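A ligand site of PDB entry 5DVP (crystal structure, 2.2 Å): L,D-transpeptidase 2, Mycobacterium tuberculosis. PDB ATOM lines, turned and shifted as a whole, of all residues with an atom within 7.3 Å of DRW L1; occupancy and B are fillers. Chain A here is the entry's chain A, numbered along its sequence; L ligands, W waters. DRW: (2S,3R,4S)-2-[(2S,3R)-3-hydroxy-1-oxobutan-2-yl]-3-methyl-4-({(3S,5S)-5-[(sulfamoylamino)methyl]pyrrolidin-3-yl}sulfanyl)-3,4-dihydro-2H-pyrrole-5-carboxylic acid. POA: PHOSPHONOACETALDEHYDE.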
ATOM      1  N   SER A 222      18.609 -13.357 -30.364  1.00  0.00           N
ATOM      2  CA  SER A 222      17.184 -13.653 -30.544  1.00  0.00           C
ATOM      3  C   SER A 222      16.417 -12.350 -30.363  1.00  0.00           C
ATOM      4  O   SER A 222      16.522 -11.720 -29.307  1.00  0.00           O
ATOM      5  CB  SER A 222      16.702 -14.700 -29.548  1.00  0.00           C
ATOM      6  OG  SER A 222      15.361 -15.073 -29.792  1.00  0.00           O
ATOM      7  N   MET A 223      15.667 -11.947 -31.391  1.00  0.00           N
ATOM      8  CA  MET A 223      14.942 -10.684 -31.344  1.00  0.00           C
ATOM      9  C   MET A 223      13.443 -10.938 -31.108  1.00  0.00           C
ATOM     10  O   MET A 223      13.061 -12.031 -30.689  1.00  0.00           O
ATOM     11  CB  MET A 223      15.210  -9.880 -32.619  1.00  0.00           C
ATOM     12  CG  MET A 223      16.659  -9.397 -32.723  1.00  0.00           C
ATOM     13  SD  MET A 223      17.036  -8.208 -34.043  1.00  0.00           S
ATOM     14  CE  MET A 223      16.951  -9.252 -35.500  1.00  0.00           C
ATOM     15  N   GLY A 224      12.596  -9.946 -31.339  1.00  0.00           N
ATOM     16  CA  GLY A 224      11.170 -10.115 -31.102  1.00  0.00           C
ATOM     17  C   GLY A 224      10.512 -11.169 -31.985  1.00  0.00           C
ATOM     18  O   GLY A 224      10.671 -11.169 -33.209  1.00  0.00           O
ATOM     19  N   LYS A 225       9.756 -12.079 -31.355  1.00  0.00           N
ATOM     20  CA  LYS A 225       8.914 -13.034 -32.078  1.00  0.00           C
ATOM     21  C   LYS A 225       7.935 -12.300 -32.980  1.00  0.00           C
ATOM     22  O   LYS A 225       7.697 -11.099 -32.788  1.00  0.00           O
ATOM     23  CB  LYS A 225       8.158 -13.959 -31.104  1.00  0.00           C
ATOM     24  CG  LYS A 225       7.287 -13.219 -30.074  1.00  0.00           C
ATOM     25  CD  LYS A 225       6.661 -14.171 -29.062  1.00  0.00           C
ATOM     26  CE  LYS A 225       5.703 -13.451 -28.128  1.00  0.00           C
ATOM     27  NZ  LYS A 225       6.363 -12.410 -27.271  1.00  0.00           N
ATOM     28  N   THR A 228       5.385 -10.002 -31.458  1.00  0.00           N
ATOM     29  CA  THR A 228       5.956  -8.803 -30.813  1.00  0.00           C
ATOM     30  C   THR A 228       7.323  -8.485 -31.435  1.00  0.00           C
ATOM     31  O   THR A 228       8.375  -8.650 -30.794  1.00  0.00           O
ATOM     32  CB  THR A 228       6.081  -8.987 -29.282  1.00  0.00           C
ATOM     33  OG1 THR A 228       6.911 -10.114 -28.959  1.00  0.00           O
ATOM     34  CG2 THR A 228       4.703  -9.204 -28.650  1.00  0.00           C
ATOM     35  N   MET A 246      13.353  -5.101 -15.751  1.00  0.00           N
ATOM     36  CA  MET A 246      12.617  -4.570 -16.886  1.00  0.00           C
ATOM     37  C   MET A 246      11.118  -4.747 -16.656  1.00  0.00           C
ATOM     38  O   MET A 246      10.592  -5.851 -16.720  1.00  0.00           O
ATOM     39  CB  MET A 246      13.062  -5.229 -18.189  1.00  0.00           C
ATOM     40  CG  MET A 246      14.476  -4.848 -18.635  1.00  0.00           C
ATOM     41  SD  MET A 246      14.839  -5.420 -20.319  1.00  0.00           S
ATOM     42  CE  MET A 246      14.162  -7.082 -20.249  1.00  0.00           C
ATOM     43  N   TYR A 251       6.798   1.067 -20.188  1.00  0.00           N
ATOM     44  CA  TYR A 251       6.709   1.322 -21.624  1.00  0.00           C
ATOM     45  C   TYR A 251       5.290   1.163 -22.157  1.00  0.00           C
ATOM     46  O   TYR A 251       5.102   0.907 -23.343  1.00  0.00           O
ATOM     47  CB  TYR A 251       7.658   0.392 -22.380  1.00  0.00           C
ATOM     48  CG  TYR A 251       8.956   0.204 -21.635  1.00  0.00           C
ATOM     49  CD1 TYR A 251       9.834   1.256 -21.448  1.00  0.00           C
ATOM     50  CD2 TYR A 251       9.293  -1.032 -21.094  1.00  0.00           C
ATOM     51  CE1 TYR A 251      11.018   1.094 -20.758  1.00  0.00           C
ATOM     52  CE2 TYR A 251      10.467  -1.208 -20.401  1.00  0.00           C
ATOM     53  CZ  TYR A 251      11.319  -0.148 -20.233  1.00  0.00           C
ATOM     54  OH  TYR A 251      12.491  -0.327 -19.531  1.00  0.00           O
ATOM     55  N   TYR A 261       5.327  -8.078 -18.953  1.00  0.00           N
ATOM     56  CA  TYR A 261       6.439  -8.808 -18.338  1.00  0.00           C
ATOM     57  C   TYR A 261       7.060  -7.972 -17.233  1.00  0.00           C
ATOM     58  O   TYR A 261       6.867  -6.751 -17.152  1.00  0.00           O
ATOM     59  CB  TYR A 261       7.506  -9.181 -19.377  1.00  0.00           C
ATOM     60  CG  TYR A 261       8.061  -8.010 -20.155  1.00  0.00           C
ATOM     61  CD1 TYR A 261       9.148  -7.273 -19.691  1.00  0.00           C
ATOM     62  CD2 TYR A 261       7.487  -7.619 -21.359  1.00  0.00           C
ATOM     63  CE1 TYR A 261       9.657  -6.185 -20.403  1.00  0.00           C
ATOM     64  CE2 TYR A 261       7.981  -6.531 -22.088  1.00  0.00           C
ATOM     65  CZ  TYR A 261       9.063  -5.822 -21.603  1.00  0.00           C
ATOM     66  OH  TYR A 261       9.540  -4.755 -22.312  1.00  0.00           O
ATOM     67  N   THR A 263      10.993  -8.631 -15.649  1.00  0.00           N
ATOM     68  CA  THR A 263      12.116  -9.559 -15.574  1.00  0.00           C
ATOM     69  C   THR A 263      13.369  -8.885 -15.062  1.00  0.00           C
ATOM     70  O   THR A 263      13.753  -7.809 -15.531  1.00  0.00           O
ATOM     71  CB  THR A 263      12.443 -10.178 -16.951  1.00  0.00           C
ATOM     72  OG1 THR A 263      11.259 -10.290 -17.741  1.00  0.00           O
ATOM     73  CG2 THR A 263      13.073 -11.552 -16.758  1.00  0.00           C
ATOM     74  N   VAL A 265      17.130  -8.677 -15.296  1.00  0.00           N
ATOM     75  CA  VAL A 265      18.128  -9.081 -16.292  1.00  0.00           C
ATOM     76  C   VAL A 265      19.450  -8.399 -16.021  1.00  0.00           C
ATOM     77  O   VAL A 265      19.524  -7.364 -15.359  1.00  0.00           O
ATOM     78  CB  VAL A 265      17.680  -8.764 -17.736  1.00  0.00           C
ATOM     79  CG1 VAL A 265      16.258  -9.274 -17.993  1.00  0.00           C
ATOM     80  CG2 VAL A 265      17.799  -7.273 -18.029  1.00  0.00           C
ATOM     81  N   SER A 274      10.959   3.024 -25.907  1.00  0.00           N
ATOM     82  CA  SER A 274       9.867   2.051 -26.009  1.00  0.00           C
ATOM     83  C   SER A 274      10.205   0.748 -25.289  1.00  0.00           C
ATOM     84  O   SER A 274       9.350  -0.134 -25.158  1.00  0.00           O
ATOM     85  CB  SER A 274       9.526   1.772 -27.473  1.00  0.00           C
ATOM     86  OG  SER A 274      10.570   1.066 -28.123  1.00  0.00           O
ATOM     87  N   GLY A 275      11.439   0.634 -24.811  1.00  0.00           N
ATOM     88  CA  GLY A 275      11.815  -0.506 -23.985  1.00  0.00           C
ATOM     89  C   GLY A 275      12.697  -1.568 -24.633  1.00  0.00           C
ATOM     90  O   GLY A 275      12.883  -2.668 -24.076  1.00  0.00           O
ATOM     91  N   VAL A 276      13.266  -1.248 -25.782  1.00  0.00           N
ATOM     92  CA  VAL A 276      14.215  -2.177 -26.380  1.00  0.00           C
ATOM     93  C   VAL A 276      15.578  -2.061 -25.703  1.00  0.00           C
ATOM     94  O   VAL A 276      16.170  -0.969 -25.607  1.00  0.00           O
ATOM     95  CB  VAL A 276      14.333  -1.960 -27.901  1.00  0.00           C
ATOM     96  CG1 VAL A 276      15.348  -2.944 -28.505  1.00  0.00           C
ATOM     97  CG2 VAL A 276      12.960  -2.138 -28.559  1.00  0.00           C
ATOM     98  N   PHE A 277      16.068  -3.207 -25.220  1.00  0.00           N
ATOM     99  CA  PHE A 277      17.391  -3.331 -24.612  1.00  0.00           C
ATOM    100  C   PHE A 277      18.207  -4.403 -25.333  1.00  0.00           C
ATOM    101  O   PHE A 277      17.648  -5.387 -25.805  1.00  0.00           O
ATOM    102  CB  PHE A 277      17.310  -3.730 -23.132  1.00  0.00           C
ATOM    103  CG  PHE A 277      16.772  -2.677 -22.204  1.00  0.00           C
ATOM    104  CD1 PHE A 277      15.419  -2.421 -22.123  1.00  0.00           C
ATOM    105  CD2 PHE A 277      17.632  -2.001 -21.339  1.00  0.00           C
ATOM    106  CE1 PHE A 277      14.925  -1.464 -21.235  1.00  0.00           C
ATOM    107  CE2 PHE A 277      17.147  -1.041 -20.448  1.00  0.00           C
ATOM    108  CZ  PHE A 277      15.786  -0.779 -20.401  1.00  0.00           C
ATOM    109  N   HIS A 279      20.591  -7.169 -23.889  1.00  0.00           N
ATOM    110  CA  HIS A 279      20.727  -7.660 -22.521  1.00  0.00           C
ATOM    111  C   HIS A 279      21.005  -9.162 -22.459  1.00  0.00           C
ATOM    112  O   HIS A 279      20.741  -9.885 -23.414  1.00  0.00           O
ATOM    113  CB  HIS A 279      19.451  -7.365 -21.733  1.00  0.00           C
ATOM    114  CG  HIS A 279      18.302  -8.233 -22.132  1.00  0.00           C
ATOM    115  ND1 HIS A 279      18.089  -9.484 -21.585  1.00  0.00           N
ATOM    116  CD2 HIS A 279      17.332  -8.065 -23.068  1.00  0.00           C
ATOM    117  CE1 HIS A 279      17.021 -10.031 -22.141  1.00  0.00           C
ATOM    118  NE2 HIS A 279      16.541  -9.189 -23.046  1.00  0.00           N
ATOM    119  N   SER A 280      21.510  -9.601 -21.308  1.00  0.00           N
ATOM    120  CA  SER A 280      21.764 -11.018 -21.066  1.00  0.00           C
ATOM    121  C   SER A 280      20.487 -11.827 -21.006  1.00  0.00           C
ATOM    122  O   SER A 280      19.568 -11.513 -20.238  1.00  0.00           O
ATOM    123  CB  SER A 280      22.542 -11.215 -19.772  1.00  0.00           C
ATOM    124  OG  SER A 280      22.663 -12.604 -19.490  1.00  0.00           O
ATOM    125  N   ALA A 281      20.432 -12.886 -21.805  1.00  0.00           N
ATOM    126  CA  ALA A 281      19.268 -13.756 -21.884  1.00  0.00           C
ATOM    127  C   ALA A 281      19.690 -15.220 -21.812  1.00  0.00           C
ATOM    128  O   ALA A 281      19.723 -15.918 -22.830  1.00  0.00           O
ATOM    129  CB  ALA A 281      18.499 -13.476 -23.155  1.00  0.00           C
ATOM    130  N   TRP A 283      18.135 -17.736 -20.719  1.00  0.00           N
ATOM    131  CA  TRP A 283      17.024 -18.628 -21.068  1.00  0.00           C
ATOM    132  C   TRP A 283      16.861 -18.915 -22.559  1.00  0.00           C
ATOM    133  O   TRP A 283      16.200 -19.880 -22.927  1.00  0.00           O
ATOM    134  CB  TRP A 283      15.708 -18.066 -20.524  1.00  0.00           C
ATOM    135  CG  TRP A 283      15.380 -16.705 -21.083  1.00  0.00           C
ATOM    136  CD1 TRP A 283      14.722 -16.420 -22.256  1.00  0.00           C
ATOM    137  CD2 TRP A 283      15.727 -15.442 -20.508  1.00  0.00           C
ATOM    138  NE1 TRP A 283      14.629 -15.060 -22.438  1.00  0.00           N
ATOM    139  CE2 TRP A 283      15.225 -14.435 -21.373  1.00  0.00           C
ATOM    140  CE3 TRP A 283      16.387 -15.061 -19.341  1.00  0.00           C
ATOM    141  CZ2 TRP A 283      15.390 -13.079 -21.101  1.00  0.00           C
ATOM    142  CZ3 TRP A 283      16.540 -13.698 -19.070  1.00  0.00           C
ATOM    143  CH2 TRP A 283      16.048 -12.728 -19.945  1.00  0.00           C
ATOM    144  N   SER A 284      17.428 -18.089 -23.436  1.00  0.00           N
ATOM    145  CA  SER A 284      17.237 -18.332 -24.877  1.00  0.00           C
ATOM    146  C   SER A 284      18.527 -18.534 -25.682  1.00  0.00           C
ATOM    147  O   SER A 284      18.518 -18.388 -26.904  1.00  0.00           O
ATOM    148  CB  SER A 284      16.461 -17.181 -25.519  1.00  0.00           C
ATOM    149  OG  SER A 284      17.167 -15.961 -25.380  1.00  0.00           O
ATOM    150  N   THR A 293      12.455 -15.015 -30.195  1.00  0.00           N
ATOM    151  CA  THR A 293      11.639 -15.452 -29.066  1.00  0.00           C
ATOM    152  C   THR A 293      11.218 -14.333 -28.104  1.00  0.00           C
ATOM    153  O   THR A 293      10.428 -14.578 -27.189  1.00  0.00           O
ATOM    154  CB  THR A 293      12.382 -16.541 -28.244  1.00  0.00           C
ATOM    155  OG1 THR A 293      13.586 -15.997 -27.695  1.00  0.00           O
ATOM    156  CG2 THR A 293      12.724 -17.773 -29.107  1.00  0.00           C
ATOM    157  N   SER A 294      11.727 -13.119 -28.276  1.00  0.00           N
ATOM    158  CA  SER A 294      11.539 -12.121 -27.217  1.00  0.00           C
ATOM    159  C   SER A 294      10.325 -11.214 -27.433  1.00  0.00           C
ATOM    160  O   SER A 294       9.548 -11.421 -28.367  1.00  0.00           O
ATOM    161  CB  SER A 294      12.803 -11.277 -27.054  1.00  0.00           C
ATOM    162  OG  SER A 294      12.827 -10.179 -27.952  1.00  0.00           O
ATOM    163  N   HIS A 295      10.171 -10.223 -26.555  1.00  0.00           N
ATOM    164  CA  HIS A 295       9.121  -9.216 -26.653  1.00  0.00           C
ATOM    165  C   HIS A 295       9.544  -8.043 -27.534  1.00  0.00           C
ATOM    166  O   HIS A 295       8.745  -7.143 -27.815  1.00  0.00           O
ATOM    167  CB  HIS A 295       8.738  -8.678 -25.269  1.00  0.00           C
ATOM    168  CG  HIS A 295       7.950  -9.650 -24.437  1.00  0.00           C
ATOM    169  ND1 HIS A 295       8.548 -10.493 -23.523  1.00  0.00           N
ATOM    170  CD2 HIS A 295       6.622  -9.897 -24.372  1.00  0.00           C
ATOM    171  CE1 HIS A 295       7.614 -11.217 -22.936  1.00  0.00           C
ATOM    172  NE2 HIS A 295       6.442 -10.887 -23.437  1.00  0.00           N
ATOM    173  N   GLY A 296      10.801  -8.045 -27.952  1.00  0.00           N
ATOM    174  CA  GLY A 296      11.293  -7.013 -28.837  1.00  0.00           C
ATOM    175  C   GLY A 296      12.742  -6.698 -28.541  1.00  0.00           C
ATOM    176  O   GLY A 296      13.432  -6.128 -29.375  1.00  0.00           O
ATOM    177  N   CYS A 297      13.189  -7.089 -27.349  1.00  0.00           N
ATOM    178  CA  CYS A 297      14.581  -6.889 -26.924  1.00  0.00           C
ATOM    179  C   CYS A 297      15.551  -7.727 -27.762  1.00  0.00           C
ATOM    180  O   CYS A 297      15.182  -8.745 -28.357  1.00  0.00           O
ATOM    181  CB  CYS A 297      14.764  -7.237 -25.441  1.00  0.00           C
ATOM    182  SG  CYS A 297      13.997  -6.062 -24.282  1.00  0.00           S
ATOM    183  N   LEU A 298      16.806  -7.292 -27.807  1.00  0.00           N
ATOM    184  CA  LEU A 298      17.833  -8.112 -28.450  1.00  0.00           C
ATOM    185  C   LEU A 298      18.469  -9.001 -27.403  1.00  0.00           C
ATOM    186  O   LEU A 298      19.373  -8.578 -26.670  1.00  0.00           O
ATOM    187  CB  LEU A 298      18.874  -7.234 -29.144  1.00  0.00           C
ATOM    188  CG  LEU A 298      18.578  -6.711 -30.559  1.00  0.00           C
ATOM    189  CD1 LEU A 298      17.270  -5.919 -30.638  1.00  0.00           C
ATOM    190  CD2 LEU A 298      19.735  -5.841 -31.057  1.00  0.00           C
ATOM    191  N   ASN A 299      17.953 -10.239 -27.311  1.00  0.00           N
ATOM    192  CA  ASN A 299      18.534 -11.262 -26.468  1.00  0.00           C
ATOM    193  C   ASN A 299      19.927 -11.639 -26.983  1.00  0.00           C
ATOM    194  O   ASN A 299      20.071 -11.957 -28.150  1.00  0.00           O
ATOM    195  CB  ASN A 299      17.658 -12.527 -26.450  1.00  0.00           C
ATOM    196  CG  ASN A 299      16.384 -12.364 -25.642  1.00  0.00           C
ATOM    197  OD1 ASN A 299      15.993 -11.256 -25.259  1.00  0.00           O
ATOM    198  ND2 ASN A 299      15.728 -13.485 -25.367  1.00  0.00           N
HETATM  199  CAB DRW L   1      13.653 -10.149 -21.832  1.00  0.00           C
HETATM  200  OAD DRW L   1      11.625  -6.303 -24.530  1.00  0.00           O
HETATM  201  CAJ DRW L   1      12.387  -7.243 -24.300  1.00  0.00           C
HETATM  202  NAN DRW L   1      11.278 -10.818 -24.048  1.00  0.00           N
HETATM  203  CAS DRW L   1      11.782 -12.029 -23.752  1.00  0.00           C
HETATM  204  CAU DRW L   1      13.281 -10.568 -23.245  1.00  0.00           C
HETATM  205  CAX DRW L   1      11.949  -8.471 -23.466  1.00  0.00           C
HETATM  206  CAY DRW L   1      12.391  -9.834 -24.048  1.00  0.00           C
HETATM  207  CAZ DRW L   1      13.077 -11.864 -23.499  1.00  0.00           C
HETATM  208  C1  POA L   2       8.037  -3.370 -24.947  1.00  0.00           C
HETATM  209  C2  POA L   2       8.790  -3.717 -26.215  1.00  0.00           C
HETATM  210  O2  POA L   2       9.907  -4.224 -26.159  1.00  0.00           O
HETATM  211  O   HOH W   1      13.245 -14.722 -24.791  1.00  0.00           O
HETATM  212  O   HOH W   2      10.624 -10.951 -20.633  1.00  0.00           O
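N of Cys 297 sits close to OAD of DRW L1 (3.3 Å). A ring nitrogen (ND1) of His 295 is in hydrogen-bond range of a nitrogen (NAN) of DRW L1 (2.8 Å). N of His 295 is in hydrogen-bond range of NAN of DRW L1 (2.8 Å). A carbon (CAJ) of DRW L1 is bonded to the side-chain sulfur (SG) of Cys 297. The side-chain hydroxyl (OH) of Tyr 261 sits at hydrogen-bond distance from an oxygen (OAD) of DRW L1 (3.4 Å).
Water W1 lies within hydrogen-bond range of NE1 of Trp 283 (2.8 Å), ND2 of Asn 299 (2.8 Å) and OG1 of Thr 293 (3.2 Å). Water W2 lies within hydrogen-bond range of OG1 of Thr 263 (3.0 Å) and NAN of DRW L1 (3.5 Å).
The backbone carbonyl oxygen of Thr 263 is in hydrogen-bond range of the backbone NH of Met 246 (2.7 Å). The side-chain hydroxyl (OG) of Ser 294 lies within hydrogen-bond range of the backbone carbonyl oxygen (O) of Cys 297 (2.8 Å). The side-chain amide oxygen (OD1) of Asn 299 sits at hydrogen-bond distance from a ring nitrogen (NE2) of His 279. The side-chain hydroxyl (OG) of Ser 294 sits at hydrogen-bond distance from the backbone NH (N) of Gly 296 (2.9 Å). O of Met 223 lies within hydrogen-bond range of N of Ser 294. N of Phe 277 lies within hydrogen-bond range of SG of Cys 297, at 3.6 Å. The backbone carbonyl oxygen of Ser 294 lies within hydrogen-bond range of the side-chain hydroxyl of Thr 228, 3.0 Å away. The backbone NH (N) of Asn 299 is in hydrogen-bond range of the backbone carbonyl oxygen (O) of Ser 222, 2.9 Å away.
Merely in contact with DRW L1: Met 246, Gly 275, His 279, Trp 283, Ser 294, Gly 296 and Asn 299. Along chain A the residues within 4 Å of DRW L1 span positions 246 to 299.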
